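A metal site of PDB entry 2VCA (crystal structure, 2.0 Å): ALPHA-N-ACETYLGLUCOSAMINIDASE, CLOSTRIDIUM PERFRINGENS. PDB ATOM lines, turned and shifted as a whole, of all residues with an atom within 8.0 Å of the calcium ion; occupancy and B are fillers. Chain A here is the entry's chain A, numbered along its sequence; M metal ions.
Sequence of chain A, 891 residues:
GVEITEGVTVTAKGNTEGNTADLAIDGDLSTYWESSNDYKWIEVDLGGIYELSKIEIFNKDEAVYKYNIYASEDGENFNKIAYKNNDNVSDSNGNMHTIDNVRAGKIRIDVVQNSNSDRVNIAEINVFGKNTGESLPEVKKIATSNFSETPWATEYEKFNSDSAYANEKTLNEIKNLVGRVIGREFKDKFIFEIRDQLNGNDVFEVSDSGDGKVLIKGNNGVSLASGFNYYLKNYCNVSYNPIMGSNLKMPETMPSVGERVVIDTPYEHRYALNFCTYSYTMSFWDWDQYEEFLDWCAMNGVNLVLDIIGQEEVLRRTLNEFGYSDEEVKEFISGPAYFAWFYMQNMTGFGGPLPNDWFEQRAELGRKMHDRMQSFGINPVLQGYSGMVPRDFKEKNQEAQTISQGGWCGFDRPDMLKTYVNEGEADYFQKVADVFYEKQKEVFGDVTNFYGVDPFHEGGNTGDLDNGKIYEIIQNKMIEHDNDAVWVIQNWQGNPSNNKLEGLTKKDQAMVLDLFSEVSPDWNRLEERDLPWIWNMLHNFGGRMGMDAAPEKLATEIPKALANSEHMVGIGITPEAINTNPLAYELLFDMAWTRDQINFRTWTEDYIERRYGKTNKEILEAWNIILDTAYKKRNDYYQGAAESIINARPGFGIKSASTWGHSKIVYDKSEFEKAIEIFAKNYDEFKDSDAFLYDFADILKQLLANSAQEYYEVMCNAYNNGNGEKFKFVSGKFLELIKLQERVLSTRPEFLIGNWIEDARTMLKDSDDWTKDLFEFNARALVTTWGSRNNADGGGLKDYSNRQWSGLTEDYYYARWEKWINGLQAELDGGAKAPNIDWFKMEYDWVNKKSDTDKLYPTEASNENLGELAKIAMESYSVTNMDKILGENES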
ATOM      1  N   THR A  20      20.136 -18.612   4.607  1.00  0.00           N
ATOM      2  CA  THR A  20      21.531 -18.922   4.729  1.00  0.00           C
ATOM      3  C   THR A  20      21.794 -20.095   5.654  1.00  0.00           C
ATOM      4  O   THR A  20      20.975 -20.434   6.455  1.00  0.00           O
ATOM      5  CB  THR A  20      22.307 -17.686   5.225  1.00  0.00           C
ATOM      6  OG1 THR A  20      21.711 -17.170   6.396  1.00  0.00           O
ATOM      7  CG2 THR A  20      22.304 -16.607   4.229  1.00  0.00           C
ATOM      8  N   ALA A  21      22.962 -20.710   5.507  1.00  0.00           N
ATOM      9  CA  ALA A  21      23.342 -21.915   6.262  1.00  0.00           C
ATOM     10  C   ALA A  21      23.181 -21.807   7.787  1.00  0.00           C
ATOM     11  O   ALA A  21      22.683 -22.739   8.427  1.00  0.00           O
ATOM     12  CB  ALA A  21      24.759 -22.338   5.902  1.00  0.00           C
ATOM     13  N   ASP A  22      23.602 -20.673   8.353  1.00  0.00           N
ATOM     14  CA  ASP A  22      23.512 -20.415   9.804  1.00  0.00           C
ATOM     15  C   ASP A  22      22.091 -20.539  10.351  1.00  0.00           C
ATOM     16  O   ASP A  22      21.898 -20.772  11.538  1.00  0.00           O
ATOM     17  CB  ASP A  22      24.095 -19.036  10.142  1.00  0.00           C
ATOM     18  CG  ASP A  22      23.406 -17.921   9.392  1.00  0.00           C
ATOM     19  OD1 ASP A  22      22.738 -17.086  10.029  1.00  0.00           O
ATOM     20  OD2 ASP A  22      23.510 -17.882   8.160  1.00  0.00           O
ATOM     21  N   LEU A  23      21.101 -20.393   9.475  1.00  0.00           N
ATOM     22  CA  LEU A  23      19.695 -20.512   9.862  1.00  0.00           C
ATOM     23  C   LEU A  23      19.279 -21.963  10.128  1.00  0.00           C
ATOM     24  O   LEU A  23      18.185 -22.208  10.658  1.00  0.00           O
ATOM     25  CB  LEU A  23      18.777 -19.836   8.831  1.00  0.00           C
ATOM     26  CG  LEU A  23      19.009 -18.324   8.609  1.00  0.00           C
ATOM     27  CD1 LEU A  23      17.974 -17.767   7.637  1.00  0.00           C
ATOM     28  CD2 LEU A  23      19.018 -17.518   9.914  1.00  0.00           C
ATOM     29  N   ALA A  24      20.141 -22.912   9.776  1.00  0.00           N
ATOM     30  CA  ALA A  24      19.922 -24.310  10.136  1.00  0.00           C
ATOM     31  C   ALA A  24      20.244 -24.584  11.610  1.00  0.00           C
ATOM     32  O   ALA A  24      19.801 -25.594  12.163  1.00  0.00           O
ATOM     33  CB  ALA A  24      20.760 -25.226   9.235  1.00  0.00           C
ATOM     34  N   ILE A  25      21.014 -23.699  12.238  1.00  0.00           N
ATOM     35  CA  ILE A  25      21.504 -23.924  13.602  1.00  0.00           C
ATOM     36  C   ILE A  25      21.257 -22.762  14.583  1.00  0.00           C
ATOM     37  O   ILE A  25      21.995 -22.597  15.558  1.00  0.00           O
ATOM     38  CB  ILE A  25      23.022 -24.308  13.611  1.00  0.00           C
ATOM     39  CG1 ILE A  25      23.858 -23.237  12.896  1.00  0.00           C
ATOM     40  CG2 ILE A  25      23.250 -25.694  13.020  1.00  0.00           C
ATOM     41  CD1 ILE A  25      25.294 -23.143  13.395  1.00  0.00           C
ATOM     42  N   ASP A  26      20.216 -21.979  14.331  1.00  0.00           N
ATOM     43  CA  ASP A  26      19.959 -20.766  15.119  1.00  0.00           C
ATOM     44  C   ASP A  26      18.937 -20.961  16.245  1.00  0.00           C
ATOM     45  O   ASP A  26      18.527 -19.996  16.886  1.00  0.00           O
ATOM     46  CB  ASP A  26      19.573 -19.581  14.221  1.00  0.00           C
ATOM     47  CG  ASP A  26      18.229 -19.764  13.537  1.00  0.00           C
ATOM     48  OD1 ASP A  26      17.690 -20.891  13.528  1.00  0.00           O
ATOM     49  OD2 ASP A  26      17.713 -18.787  12.968  1.00  0.00           O
ATOM     50  N   GLY A  27      18.529 -22.215  16.476  1.00  0.00           N
ATOM     51  CA  GLY A  27      17.563 -22.551  17.532  1.00  0.00           C
ATOM     52  C   GLY A  27      16.130 -22.154  17.228  1.00  0.00           C
ATOM     53  O   GLY A  27      15.243 -22.325  18.073  1.00  0.00           O
ATOM     54  N   ASP A  28      15.906 -21.656  16.019  1.00  0.00           N
ATOM     55  CA  ASP A  28      14.611 -21.114  15.602  1.00  0.00           C
ATOM     56  C   ASP A  28      14.012 -22.005  14.514  1.00  0.00           C
ATOM     57  O   ASP A  28      14.577 -22.129  13.424  1.00  0.00           O
ATOM     58  CB  ASP A  28      14.804 -19.689  15.080  1.00  0.00           C
ATOM     59  CG  ASP A  28      13.498 -18.907  14.953  1.00  0.00           C
ATOM     60  OD1 ASP A  28      12.402 -19.513  14.882  1.00  0.00           O
ATOM     61  OD2 ASP A  28      13.572 -17.659  14.908  1.00  0.00           O
ATOM     62  N   LEU A  29      12.873 -22.615  14.818  1.00  0.00           N
ATOM     63  CA  LEU A  29      12.201 -23.515  13.886  1.00  0.00           C
ATOM     64  C   LEU A  29      11.567 -22.792  12.691  1.00  0.00           C
ATOM     65  O   LEU A  29      11.227 -23.430  11.689  1.00  0.00           O
ATOM     66  CB  LEU A  29      11.152 -24.347  14.618  1.00  0.00           C
ATOM     67  CG  LEU A  29      11.446 -25.802  14.978  1.00  0.00           C
ATOM     68  CD1 LEU A  29      12.897 -26.073  15.341  1.00  0.00           C
ATOM     69  CD2 LEU A  29      10.545 -26.247  16.098  1.00  0.00           C
ATOM     70  N   SER A  30      11.432 -21.481  12.795  1.00  0.00           N
ATOM     71  CA  SER A  30      10.774 -20.694  11.753  1.00  0.00           C
ATOM     72  C   SER A  30      11.734 -20.144  10.693  1.00  0.00           C
ATOM     73  O   SER A  30      11.308 -19.551   9.717  1.00  0.00           O
ATOM     74  CB  SER A  30       9.947 -19.556  12.382  1.00  0.00           C
ATOM     75  OG  SER A  30      10.793 -18.592  12.966  1.00  0.00           O
ATOM     76  N   THR A  31      13.041 -20.353  10.906  1.00  0.00           N
ATOM     77  CA  THR A  31      14.057 -19.936   9.947  1.00  0.00           C
ATOM     78  C   THR A  31      14.796 -21.177   9.437  1.00  0.00           C
ATOM     79  O   THR A  31      14.936 -22.149  10.177  1.00  0.00           O
ATOM     80  CB  THR A  31      15.088 -18.972  10.572  1.00  0.00           C
ATOM     81  OG1 THR A  31      15.794 -19.645  11.617  1.00  0.00           O
ATOM     82  CG2 THR A  31      14.413 -17.717  11.128  1.00  0.00           C
ATOM     83  N   TYR A  32      15.244 -21.141   8.183  1.00  0.00           N
ATOM     84  CA  TYR A  32      15.834 -22.312   7.546  1.00  0.00           C
ATOM     85  C   TYR A  32      16.896 -21.914   6.529  1.00  0.00           C
ATOM     86  O   TYR A  32      16.741 -20.925   5.805  1.00  0.00           O
ATOM     87  CB  TYR A  32      14.752 -23.154   6.869  1.00  0.00           C
ATOM     88  CG  TYR A  32      13.890 -22.383   5.906  1.00  0.00           C
ATOM     89  CD1 TYR A  32      12.742 -21.736   6.329  1.00  0.00           C
ATOM     90  CD2 TYR A  32      14.222 -22.301   4.555  1.00  0.00           C
ATOM     91  CE1 TYR A  32      11.945 -21.024   5.449  1.00  0.00           C
ATOM     92  CE2 TYR A  32      13.441 -21.595   3.673  1.00  0.00           C
ATOM     93  CZ  TYR A  32      12.305 -20.956   4.116  1.00  0.00           C
ATOM     94  OH  TYR A  32      11.511 -20.253   3.235  1.00  0.00           O
ATOM     95  N   TRP A  33      17.982 -22.682   6.471  1.00  0.00           N
ATOM     96  CA  TRP A  33      18.744 -22.843   5.241  1.00  0.00           C
ATOM     97  C   TRP A  33      17.871 -23.426   4.127  1.00  0.00           C
ATOM     98  O   TRP A  33      17.024 -24.288   4.380  1.00  0.00           O
ATOM     99  CB  TRP A  33      19.967 -23.727   5.478  1.00  0.00           C
ATOM    100  CG  TRP A  33      20.675 -24.124   4.220  1.00  0.00           C
ATOM    101  CD1 TRP A  33      21.459 -23.331   3.434  1.00  0.00           C
ATOM    102  CD2 TRP A  33      20.655 -25.413   3.596  1.00  0.00           C
ATOM    103  NE1 TRP A  33      21.936 -24.050   2.367  1.00  0.00           N
ATOM    104  CE2 TRP A  33      21.456 -25.329   2.446  1.00  0.00           C
ATOM    105  CE3 TRP A  33      20.046 -26.632   3.904  1.00  0.00           C
ATOM    106  CZ2 TRP A  33      21.658 -26.421   1.593  1.00  0.00           C
ATOM    107  CZ3 TRP A  33      20.249 -27.713   3.065  1.00  0.00           C
ATOM    108  CH2 TRP A  33      21.051 -27.599   1.920  1.00  0.00           C
ATOM    109  N   PHE A  58      14.850 -31.009  11.784  1.00  0.00           N
ATOM    110  CA  PHE A  58      13.578 -30.381  11.482  1.00  0.00           C
ATOM    111  C   PHE A  58      13.620 -29.769  10.096  1.00  0.00           C
ATOM    112  O   PHE A  58      14.619 -29.158   9.709  1.00  0.00           O
ATOM    113  CB  PHE A  58      13.241 -29.281  12.502  1.00  0.00           C
ATOM    114  CG  PHE A  58      13.069 -29.789  13.915  1.00  0.00           C
ATOM    115  CD1 PHE A  58      11.802 -30.083  14.404  1.00  0.00           C
ATOM    116  CD2 PHE A  58      14.172 -29.949  14.742  1.00  0.00           C
ATOM    117  CE1 PHE A  58      11.638 -30.547  15.707  1.00  0.00           C
ATOM    118  CE2 PHE A  58      14.016 -30.412  16.051  1.00  0.00           C
ATOM    119  CZ  PHE A  58      12.747 -30.706  16.526  1.00  0.00           C
ATOM    120  N   ILE A 122      16.748 -27.290   5.717  1.00  0.00           N
ATOM    121  CA  ILE A 122      16.843 -27.728   7.104  1.00  0.00           C
ATOM    122  C   ILE A 122      16.465 -26.533   7.977  1.00  0.00           C
ATOM    123  O   ILE A 122      17.134 -25.488   7.951  1.00  0.00           O
ATOM    124  CB  ILE A 122      18.265 -28.271   7.450  1.00  0.00           C
ATOM    125  CG1 ILE A 122      18.514 -29.610   6.746  1.00  0.00           C
ATOM    126  CG2 ILE A 122      18.412 -28.452   8.965  1.00  0.00           C
ATOM    127  CD1 ILE A 122      19.977 -29.984   6.585  1.00  0.00           C
ATOM    128  N   ALA A 123      15.369 -26.668   8.720  1.00  0.00           N
ATOM    129  CA  ALA A 123      14.921 -25.633   9.653  1.00  0.00           C
ATOM    130  C   ALA A 123      15.817 -25.609  10.884  1.00  0.00           C
ATOM    131  O   ALA A 123      16.303 -24.550  11.262  1.00  0.00           O
ATOM    132  CB  ALA A 123      13.464 -25.845  10.050  1.00  0.00           C
ATOM    133  N   GLU A 124      16.028 -26.779  11.481  1.00  0.00           N
ATOM    134  CA  GLU A 124      16.946 -26.924  12.613  1.00  0.00           C
ATOM    135  C   GLU A 124      17.633 -28.286  12.610  1.00  0.00           C
ATOM    136  O   GLU A 124      17.058 -29.272  12.159  1.00  0.00           O
ATOM    137  CB  GLU A 124      16.228 -26.735  13.964  1.00  0.00           C
ATOM    138  CG  GLU A 124      16.049 -25.284  14.417  1.00  0.00           C
ATOM    139  CD  GLU A 124      17.348 -24.508  14.484  1.00  0.00           C
ATOM    140  OE1 GLU A 124      18.228 -24.863  15.297  1.00  0.00           O
ATOM    141  OE2 GLU A 124      17.485 -23.525  13.739  1.00  0.00           O
ATOM    142  N   ILE A 125      18.852 -28.303  13.113  1.00  0.00           N
ATOM    143  CA  ILE A 125      19.542 -29.555  13.400  1.00  0.00           C
ATOM    144  C   ILE A 125      20.161 -29.505  14.800  1.00  0.00           C
ATOM    145  O   ILE A 125      20.943 -28.603  15.110  1.00  0.00           O
ATOM    146  CB  ILE A 125      20.614 -29.923  12.323  1.00  0.00           C
ATOM    147  CG1 ILE A 125      21.396 -31.167  12.760  1.00  0.00           C
ATOM    148  CG2 ILE A 125      21.545 -28.745  12.033  1.00  0.00           C
ATOM    149  CD1 ILE A 125      22.140 -31.866  11.647  1.00  0.00           C
HETATM  150 CA    CA M   1      16.415 -22.290  12.074  1.00  0.00          CA
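The side-chain carboxylate (OD1) of Asp 28 is in hydrogen-bond range of the side-chain hydroxyl (OG) of Ser 30 (2.7 Å). OE1 of Glu 124 is in hydrogen-bond range of N of Gly 27 (2.9 Å). O of Glu 124 is in hydrogen-bond range of N of Phe 58, at 2.8 Å. The backbone NH (N) of Ala 123 lies within hydrogen-bond range of the backbone carbonyl oxygen (O) of Phe 58, at 2.8 Å.
Within 4 Å of the calcium ion: Leu 23, Asp 26, Asp 28, Thr 31, Ala 123 and Glu 124. Along chain A the residues within 4 Å of the calcium ion span positions 23 to 124. The nearest printed residue that does not touch the calcium ion is Tyr 32 (4.2 Å).
O of Leu 23 binds the calcium ion, at 2.3 Å. The backbone carbonyl oxygen (O) of Asp 28 is bound to the calcium ion (2.3 Å). OE2 of Glu 124 binds the calcium ion, 2.3 Å away. OD1 of Asp 26 is bound to the calcium ion, 2.4 Å away. The calcium ion is bound by the backbone carbonyl oxygen (O) of Ala 123. O of Thr 31 is bound to the calcium ion (2.4 Å). OG1 of Thr 31 is bound to the calcium ion, at 2.8 Å.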
